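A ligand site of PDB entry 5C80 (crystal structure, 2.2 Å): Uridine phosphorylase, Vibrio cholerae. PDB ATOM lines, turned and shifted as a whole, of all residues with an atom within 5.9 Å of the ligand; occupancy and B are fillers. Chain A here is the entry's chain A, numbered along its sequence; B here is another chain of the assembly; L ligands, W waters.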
ATOM      1  N   GLY A  25     -17.169  16.820  22.110  1.00  0.00           N
ATOM      2  CA  GLY A  25     -15.974  16.109  21.709  1.00  0.00           C
ATOM      3  C   GLY A  25     -15.738  16.217  20.220  1.00  0.00           C
ATOM      4  O   GLY A  25     -14.605  16.354  19.771  1.00  0.00           O
ATOM      5  N   GLY A  67     -12.111  17.194  20.938  1.00  0.00           N
ATOM      6  CA  GLY A  67     -11.527  15.964  20.422  1.00  0.00           C
ATOM      7  C   GLY A  67     -11.725  14.869  21.452  1.00  0.00           C
ATOM      8  O   GLY A  67     -12.289  15.094  22.530  1.00  0.00           O
ATOM      9  N   ILE A  68     -11.240  13.673  21.128  1.00  0.00           N
ATOM     10  CA  ILE A  68     -11.359  12.550  22.037  1.00  0.00           C
ATOM     11  C   ILE A  68     -10.206  12.607  23.026  1.00  0.00           C
ATOM     12  O   ILE A  68      -9.058  12.751  22.615  1.00  0.00           O
ATOM     13  CB  ILE A  68     -11.299  11.210  21.269  1.00  0.00           C
ATOM     14  CG1 ILE A  68     -12.522  11.069  20.356  1.00  0.00           C
ATOM     15  CG2 ILE A  68     -11.135  10.043  22.239  1.00  0.00           C
ATOM     16  CD1 ILE A  68     -12.511   9.861  19.438  1.00  0.00           C
ATOM     17  N   GLY A  69     -10.518  12.497  24.308  1.00  0.00           N
ATOM     18  CA  GLY A  69      -9.493  12.317  25.340  1.00  0.00           C
ATOM     19  C   GLY A  69      -9.181  13.569  26.153  1.00  0.00           C
ATOM     20  O   GLY A  69      -9.413  14.689  25.715  1.00  0.00           O
ATOM     21  N   ARG A  90     -19.648  20.382  29.083  1.00  0.00           N
ATOM     22  CA  ARG A  90     -19.393  19.330  28.078  1.00  0.00           C
ATOM     23  C   ARG A  90     -20.667  18.548  27.760  1.00  0.00           C
ATOM     24  O   ARG A  90     -21.429  18.196  28.649  1.00  0.00           O
ATOM     25  CB  ARG A  90     -18.279  18.366  28.532  1.00  0.00           C
ATOM     26  CG  ARG A  90     -18.286  17.005  27.827  1.00  0.00           C
ATOM     27  CD  ARG A  90     -17.136  16.090  28.263  1.00  0.00           C
ATOM     28  NE  ARG A  90     -17.522  14.676  28.239  1.00  0.00           N
ATOM     29  CZ  ARG A  90     -17.505  13.882  27.170  1.00  0.00           C
ATOM     30  NH1 ARG A  90     -17.897  12.625  27.280  1.00  0.00           N
ATOM     31  NH2 ARG A  90     -17.086  14.336  25.988  1.00  0.00           N
ATOM     32  N   THR A  93     -21.008  11.694  24.085  1.00  0.00           N
ATOM     33  CA  THR A  93     -21.675  10.409  23.896  1.00  0.00           C
ATOM     34  C   THR A  93     -21.175   9.492  25.011  1.00  0.00           C
ATOM     35  O   THR A  93     -20.125   9.766  25.611  1.00  0.00           O
ATOM     36  CB  THR A  93     -21.393   9.842  22.486  1.00  0.00           C
ATOM     37  OG1 THR A  93     -19.995   9.615  22.329  1.00  0.00           O
ATOM     38  CG2 THR A  93     -21.843  10.883  21.414  1.00  0.00           C
ATOM     39  N   THR A  94     -21.942   8.439  25.325  1.00  0.00           N
ATOM     40  CA  THR A  94     -21.547   7.514  26.396  1.00  0.00           C
ATOM     41  C   THR A  94     -22.093   6.096  26.271  1.00  0.00           C
ATOM     42  O   THR A  94     -23.171   5.864  25.690  1.00  0.00           O
ATOM     43  CB  THR A  94     -21.886   8.046  27.807  1.00  0.00           C
ATOM     44  OG1 THR A  94     -21.221   7.239  28.785  1.00  0.00           O
ATOM     45  CG2 THR A  94     -23.394   7.999  28.068  1.00  0.00           C
ATOM     46  N   GLY A  95     -21.345   5.169  26.857  1.00  0.00           N
ATOM     47  CA  GLY A  95     -21.740   3.777  26.966  1.00  0.00           C
ATOM     48  C   GLY A  95     -22.162   3.370  28.373  1.00  0.00           C
ATOM     49  O   GLY A  95     -21.334   3.205  29.256  1.00  0.00           O
ATOM     50  N   ALA A  96     -23.461   3.182  28.564  1.00  0.00           N
ATOM     51  CA  ALA A  96     -23.983   2.734  29.833  1.00  0.00           C
ATOM     52  C   ALA A  96     -23.471   1.342  30.173  1.00  0.00           C
ATOM     53  O   ALA A  96     -23.169   0.522  29.287  1.00  0.00           O
ATOM     54  CB  ALA A  96     -25.502   2.737  29.804  1.00  0.00           C
ATOM     55  N   THR A 160      -8.703   5.088  27.420  1.00  0.00           N
ATOM     56  CA  THR A 160      -8.871   4.282  26.212  1.00  0.00           C
ATOM     57  C   THR A 160     -10.335   3.897  25.959  1.00  0.00           C
ATOM     58  O   THR A 160     -11.134   3.789  26.890  1.00  0.00           O
ATOM     59  CB  THR A 160      -8.058   2.956  26.255  1.00  0.00           C
ATOM     60  OG1 THR A 160      -8.643   2.036  27.195  1.00  0.00           O
ATOM     61  CG2 THR A 160      -6.570   3.196  26.538  1.00  0.00           C
ATOM     62  N   PHE A 161     -10.650   3.658  24.691  1.00  0.00           N
ATOM     63  CA  PHE A 161     -12.000   3.223  24.307  1.00  0.00           C
ATOM     64  C   PHE A 161     -12.122   1.736  24.530  1.00  0.00           C
ATOM     65  O   PHE A 161     -13.207   1.233  24.799  1.00  0.00           O
ATOM     66  CB  PHE A 161     -12.251   3.562  22.828  1.00  0.00           C
ATOM     67  CG  PHE A 161     -13.637   3.257  22.350  1.00  0.00           C
ATOM     68  CD1 PHE A 161     -14.655   4.207  22.466  1.00  0.00           C
ATOM     69  CD2 PHE A 161     -13.938   2.031  21.764  1.00  0.00           C
ATOM     70  CE1 PHE A 161     -15.944   3.918  22.013  1.00  0.00           C
ATOM     71  CE2 PHE A 161     -15.218   1.744  21.312  1.00  0.00           C
ATOM     72  CZ  PHE A 161     -16.227   2.687  21.447  1.00  0.00           C
ATOM     73  N   GLN A 165     -12.177   0.277  28.891  1.00  0.00           N
ATOM     74  CA  GLN A 165     -13.623   0.065  28.983  1.00  0.00           C
ATOM     75  C   GLN A 165     -13.920  -1.447  28.914  1.00  0.00           C
ATOM     76  O   GLN A 165     -15.031  -1.870  28.640  1.00  0.00           O
ATOM     77  CB  GLN A 165     -14.362   0.906  27.906  1.00  0.00           C
ATOM     78  CG  GLN A 165     -13.942   2.370  27.935  1.00  0.00           C
ATOM     79  CD  GLN A 165     -14.839   3.317  27.138  1.00  0.00           C
ATOM     80  OE1 GLN A 165     -15.968   2.986  26.740  1.00  0.00           O
ATOM     81  NE2 GLN A 165     -14.334   4.523  26.897  1.00  0.00           N
ATOM     82  N   ARG A 167     -13.213  -3.822  26.724  1.00  0.00           N
ATOM     83  CA  ARG A 167     -13.611  -4.436  25.453  1.00  0.00           C
ATOM     84  C   ARG A 167     -12.615  -5.519  25.069  1.00  0.00           C
ATOM     85  O   ARG A 167     -11.407  -5.259  25.043  1.00  0.00           O
ATOM     86  CB  ARG A 167     -13.692  -3.386  24.340  1.00  0.00           C
ATOM     87  CG  ARG A 167     -14.897  -2.481  24.456  1.00  0.00           C
ATOM     88  CD  ARG A 167     -15.050  -1.531  23.288  1.00  0.00           C
ATOM     89  NE  ARG A 167     -16.424  -1.036  23.301  1.00  0.00           N
ATOM     90  CZ  ARG A 167     -16.840   0.094  23.877  1.00  0.00           C
ATOM     91  NH1 ARG A 167     -15.972   0.936  24.471  1.00  0.00           N
ATOM     92  NH2 ARG A 167     -18.120   0.388  23.828  1.00  0.00           N
ATOM     93  N   PHE A 194     -19.529   4.842  30.838  1.00  0.00           N
ATOM     94  CA  PHE A 194     -18.136   4.856  30.465  1.00  0.00           C
ATOM     95  C   PHE A 194     -18.057   6.003  29.443  1.00  0.00           C
ATOM     96  O   PHE A 194     -18.980   6.185  28.653  1.00  0.00           O
ATOM     97  CB  PHE A 194     -17.761   3.551  29.744  1.00  0.00           C
ATOM     98  CG  PHE A 194     -17.041   2.515  30.587  1.00  0.00           C
ATOM     99  CD1 PHE A 194     -15.876   2.823  31.300  1.00  0.00           C
ATOM    100  CD2 PHE A 194     -17.468   1.181  30.567  1.00  0.00           C
ATOM    101  CE1 PHE A 194     -15.212   1.851  32.038  1.00  0.00           C
ATOM    102  CE2 PHE A 194     -16.800   0.192  31.296  1.00  0.00           C
ATOM    103  CZ  PHE A 194     -15.672   0.526  32.031  1.00  0.00           C
ATOM    104  N   GLU A 195     -16.936   6.708  29.422  1.00  0.00           N
ATOM    105  CA  GLU A 195     -16.844   7.983  28.744  1.00  0.00           C
ATOM    106  C   GLU A 195     -15.310   8.316  28.808  1.00  0.00           C
ATOM    107  O   GLU A 195     -14.575   7.623  29.510  1.00  0.00           O
ATOM    108  CB  GLU A 195     -17.804   8.894  29.516  1.00  0.00           C
ATOM    109  CG  GLU A 195     -17.740  10.388  29.349  1.00  0.00           C
ATOM    110  CD  GLU A 195     -16.573  11.006  30.050  1.00  0.00           C
ATOM    111  OE1 GLU A 195     -15.985  10.378  30.978  1.00  0.00           O
ATOM    112  OE2 GLU A 195     -16.242  12.130  29.657  1.00  0.00           O
ATOM    113  N   MET A 196     -14.820   9.307  28.078  1.00  0.00           N
ATOM    114  CA  MET A 196     -13.357   9.499  28.033  1.00  0.00           C
ATOM    115  C   MET A 196     -12.805  10.876  28.406  1.00  0.00           C
ATOM    116  O   MET A 196     -11.587  11.082  28.355  1.00  0.00           O
ATOM    117  CB  MET A 196     -12.804   9.076  26.665  1.00  0.00           C
ATOM    118  CG  MET A 196     -12.903   7.577  26.368  1.00  0.00           C
ATOM    119  SD  MET A 196     -12.422   7.128  24.704  1.00  0.00           S
ATOM    120  CE  MET A 196     -10.673   7.460  24.667  1.00  0.00           C
ATOM    121  N   GLU A 197     -13.660  11.823  28.776  1.00  0.00           N
ATOM    122  CA  GLU A 197     -13.183  13.209  28.915  1.00  0.00           C
ATOM    123  C   GLU A 197     -13.455  13.826  30.272  1.00  0.00           C
ATOM    124  O   GLU A 197     -12.792  14.810  30.634  1.00  0.00           O
ATOM    125  CB  GLU A 197     -13.785  14.109  27.819  1.00  0.00           C
ATOM    126  CG  GLU A 197     -13.268  13.842  26.416  1.00  0.00           C
ATOM    127  CD  GLU A 197     -13.946  12.645  25.722  1.00  0.00           C
ATOM    128  OE1 GLU A 197     -15.017  12.177  26.178  1.00  0.00           O
ATOM    129  OE2 GLU A 197     -13.389  12.167  24.720  1.00  0.00           O
ATOM    130  N   ILE A 219     -25.313   6.362  23.724  1.00  0.00           N
ATOM    131  CA  ILE A 219     -25.337   5.834  22.372  1.00  0.00           C
ATOM    132  C   ILE A 219     -25.133   4.318  22.364  1.00  0.00           C
ATOM    133  O   ILE A 219     -25.333   3.668  21.333  1.00  0.00           O
ATOM    134  CB  ILE A 219     -24.311   6.543  21.453  1.00  0.00           C
ATOM    135  CG1 ILE A 219     -22.858   6.321  21.928  1.00  0.00           C
ATOM    136  CG2 ILE A 219     -24.666   8.021  21.322  1.00  0.00           C
ATOM    137  CD1 ILE A 219     -21.807   6.432  20.834  1.00  0.00           C
ATOM    138  N   ILE A 220     -24.772   3.745  23.509  1.00  0.00           N
ATOM    139  CA  ILE A 220     -24.490   2.321  23.595  1.00  0.00           C
ATOM    140  C   ILE A 220     -24.682   1.844  25.025  1.00  0.00           C
ATOM    141  O   ILE A 220     -24.446   2.610  25.971  1.00  0.00           O
ATOM    142  CB  ILE A 220     -23.066   2.016  23.053  1.00  0.00           C
ATOM    143  CG1 ILE A 220     -23.000   0.673  22.317  1.00  0.00           C
ATOM    144  CG2 ILE A 220     -21.996   2.099  24.118  1.00  0.00           C
ATOM    145  CD1 ILE A 220     -22.036   0.673  21.140  1.00  0.00           C
ATOM    146  N   ARG A 222     -23.484  -1.554  27.345  1.00  0.00           N
ATOM    147  CA  ARG A 222     -22.532  -2.674  27.364  1.00  0.00           C
ATOM    148  C   ARG A 222     -23.109  -4.021  27.844  1.00  0.00           C
ATOM    149  O   ARG A 222     -22.455  -5.062  27.729  1.00  0.00           O
ATOM    150  CB  ARG A 222     -21.283  -2.296  28.151  1.00  0.00           C
ATOM    151  CG  ARG A 222     -20.576  -1.041  27.610  1.00  0.00           C
ATOM    152  CD  ARG A 222     -19.847  -1.307  26.308  1.00  0.00           C
ATOM    153  NE  ARG A 222     -19.009  -2.507  26.427  1.00  0.00           N
ATOM    154  CZ  ARG A 222     -17.821  -2.513  27.028  1.00  0.00           C
ATOM    155  NH1 ARG A 222     -17.346  -1.366  27.518  1.00  0.00           N
ATOM    156  NH2 ARG A 222     -17.120  -3.650  27.126  1.00  0.00           N
ATOM    157  N   PHE B   6     -15.256   1.150  14.238  1.00  0.00           N
ATOM    158  CA  PHE B   6     -16.092   2.179  14.863  1.00  0.00           C
ATOM    159  C   PHE B   6     -15.760   3.650  14.521  1.00  0.00           C
ATOM    160  O   PHE B   6     -16.663   4.403  14.141  1.00  0.00           O
ATOM    161  CB  PHE B   6     -16.101   2.001  16.397  1.00  0.00           C
ATOM    162  CG  PHE B   6     -17.203   2.745  17.088  1.00  0.00           C
ATOM    163  CD1 PHE B   6     -18.434   2.133  17.339  1.00  0.00           C
ATOM    164  CD2 PHE B   6     -17.024   4.066  17.501  1.00  0.00           C
ATOM    165  CE1 PHE B   6     -19.461   2.814  17.980  1.00  0.00           C
ATOM    166  CE2 PHE B   6     -18.042   4.756  18.148  1.00  0.00           C
ATOM    167  CZ  PHE B   6     -19.261   4.128  18.391  1.00  0.00           C
ATOM    168  N   HIS B   7     -14.516   4.079  14.694  1.00  0.00           N
ATOM    169  CA  HIS B   7     -14.190   5.507  14.531  1.00  0.00           C
ATOM    170  C   HIS B   7     -13.676   5.889  13.140  1.00  0.00           C
ATOM    171  O   HIS B   7     -14.039   6.942  12.605  1.00  0.00           O
ATOM    172  CB  HIS B   7     -13.204   5.944  15.579  1.00  0.00           C
ATOM    173  CG  HIS B   7     -13.756   5.927  16.972  1.00  0.00           C
ATOM    174  ND1 HIS B   7     -13.561   4.865  17.829  1.00  0.00           N
ATOM    175  CD2 HIS B   7     -14.508   6.827  17.638  1.00  0.00           C
ATOM    176  CE1 HIS B   7     -14.149   5.129  18.980  1.00  0.00           C
ATOM    177  NE2 HIS B   7     -14.736   6.316  18.892  1.00  0.00           N
ATOM    178  N   ARG B  47     -14.183  13.043  12.841  1.00  0.00           N
ATOM    179  CA  ARG B  47     -13.542  13.566  14.046  1.00  0.00           C
ATOM    180  C   ARG B  47     -12.097  14.005  13.721  1.00  0.00           C
ATOM    181  O   ARG B  47     -11.845  14.552  12.654  1.00  0.00           O
ATOM    182  CB  ARG B  47     -13.598  12.485  15.147  1.00  0.00           C
ATOM    183  CG  ARG B  47     -14.995  12.098  15.613  1.00  0.00           C
ATOM    184  CD  ARG B  47     -14.922  11.274  16.885  1.00  0.00           C
ATOM    185  NE  ARG B  47     -16.212  11.097  17.585  1.00  0.00           N
ATOM    186  CZ  ARG B  47     -16.603  11.795  18.663  1.00  0.00           C
ATOM    187  NH1 ARG B  47     -15.855  12.778  19.175  1.00  0.00           N
ATOM    188  NH2 ARG B  47     -17.775  11.536  19.229  1.00  0.00           N
ATOM    189  N   ILE B  75      -7.123   4.585  19.969  1.00  0.00           N
ATOM    190  CA  ILE B  75      -8.255   4.222  19.129  1.00  0.00           C
ATOM    191  C   ILE B  75      -7.800   3.992  17.696  1.00  0.00           C
ATOM    192  O   ILE B  75      -8.147   2.982  17.092  1.00  0.00           O
ATOM    193  CB  ILE B  75      -9.360   5.300  19.158  1.00  0.00           C
ATOM    194  CG1 ILE B  75     -10.073   5.239  20.510  1.00  0.00           C
ATOM    195  CG2 ILE B  75     -10.342   5.078  18.017  1.00  0.00           C
ATOM    196  CD1 ILE B  75     -10.967   6.437  20.767  1.00  0.00           C
HETATM  197  N1  LIG L   1     -17.721   6.986  24.433  1.00  0.00           N
HETATM  198  C1  LIG L   1     -16.971   6.047  25.181  1.00  0.00           C
HETATM  199  N2  LIG L   1     -17.455   4.803  25.371  1.00  0.00           N
HETATM  200  C2  LIG L   1     -18.623   4.407  24.860  1.00  0.00           C
HETATM  201  C3  LIG L   1     -19.375   5.296  24.098  1.00  0.00           C
HETATM  202  C4  LIG L   1     -18.904   6.583  23.885  1.00  0.00           C
HETATM  203  O1  LIG L   1     -15.864   6.350  25.698  1.00  0.00           O
HETATM  204  O2  LIG L   1     -19.000   3.208  25.045  1.00  0.00           O
HETATM  205  C5  LIG L   1     -17.320   8.376  24.099  1.00  0.00           C
HETATM  206  C6  LIG L   1     -16.038   9.030  24.656  1.00  0.00           C
HETATM  207  C7  LIG L   1     -15.340   9.645  23.436  1.00  0.00           C
HETATM  208  C8  LIG L   1     -16.108   9.174  22.216  1.00  0.00           C
HETATM  209  O3  LIG L   1     -16.305  10.097  25.579  1.00  0.00           O
HETATM  210  O4  LIG L   1     -15.520  11.046  23.366  1.00  0.00           O
HETATM  211  O5  LIG L   1     -17.074   8.256  22.687  1.00  0.00           O
HETATM  212  C9  LIG L   1     -15.236   8.497  21.165  1.00  0.00           C
HETATM  213  O6  LIG L   1     -16.088   7.887  20.196  1.00  0.00           O
HETATM  214  O   HOH W   1     -19.089   8.518  20.005  1.00  0.00           O
HETATM  215  O   HOH W   2     -17.973  12.496  23.830  1.00  0.00           O
HETATM  216  O   HOH W   3     -18.266   1.495  27.252  1.00  0.00           O
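Residues that only touch the ligand: Ile 68 (3.5 Å), Thr 94 (3.6 Å), Gly 95 (3.4 Å), Phe 161 (3.8 Å), Phe 194 (3.9 Å), Glu 195 (3.6 Å) and Ile 220 (3.3 Å). Hydrophobic or aromatic side chains within 4 Å of the ligand: Ile 68, Phe 161, Met 196, Ile 220 and His 7 of chain B. Within 4 Å of the ligand: Ile 68, Arg 90, Thr 93, Thr 94, Gly 95, Phe 161, Gln 165, Arg 167, Phe 194, Glu 195, Met 196, Glu 197, Ile 220 and His 7 of chain B. The nearest printed residue that does not touch the ligand is Arg 47 of chain B (4.1 Å).
An oxygen (O6) of the ligand lies within hydrogen-bond range of a ring nitrogen (NE2) of His 7 of chain B (2.4 Å). An oxygen (O2) of the ligand sits at hydrogen-bond distance from the guanidinium group of Arg 167 (3.2 Å). An oxygen (O3) of the ligand lies within hydrogen-bond range of the side-chain carboxylate (OE1) of Glu 197 (2.5 Å). An oxygen (O3) of the ligand is in hydrogen-bond range of the guanidinium group (NH1) of Arg 90. An oxygen (O1) of the ligand sits at hydrogen-bond distance from the side-chain amide nitrogen (NE2) of Gln 165, at 2.7 Å. The backbone NH (N) of Met 196 lies within hydrogen-bond range of an oxygen (O3) of the ligand. The side-chain hydroxyl of Thr 93 lies within hydrogen-bond range of an oxygen (O5) of the ligand (3.2 Å).
The backbone carbonyl oxygen (O) of Gly 95 is in hydrogen-bond range of the backbone NH (N) of Phe 194 (2.9 Å). The backbone carbonyl oxygen of Thr 160 lies within hydrogen-bond range of the side-chain amide nitrogen of Gln 165 (3.3 Å). The backbone NH of Ile 220 lies within hydrogen-bond range of the backbone carbonyl oxygen of Thr 94 (3.4 Å). The backbone NH (N) of Glu 197 sits at hydrogen-bond distance from the side-chain carboxylate (OE2) of Glu 195. The backbone NH (N) of Ile 219 is in hydrogen-bond range of the backbone carbonyl oxygen (O) of Thr 94 (2.9 Å). NH2 of Arg 90 lies within salt-bridge range of OE1 of Glu 197 (3.0 Å). OE2 of Glu 197 sits at hydrogen-bond distance from N of Gly 69 (2.9 Å). The backbone carbonyl oxygen (O) of Phe 161 lies within hydrogen-bond range of the guanidinium group (NH1) of Arg 167.
Water W2 lies within hydrogen-bond range of an oxygen (O4) of the ligand (2.9 Å), the guanidinium group (NH2) of Arg 90 (3.0 Å) and the backbone NH (N) of Thr 93 (3.1 Å). Water W3 lies within hydrogen-bond range of the side-chain amide oxygen (OE1) of Gln 165, an oxygen (O2) of the ligand and the guanidinium group (NH1) of Arg 222. Water W1 lies within hydrogen-bond range of OG1 of Thr 93 (2.7 Å), O6 of the ligand (3.1 Å) and NH2 of Arg 47 of chain B (3.4 Å).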
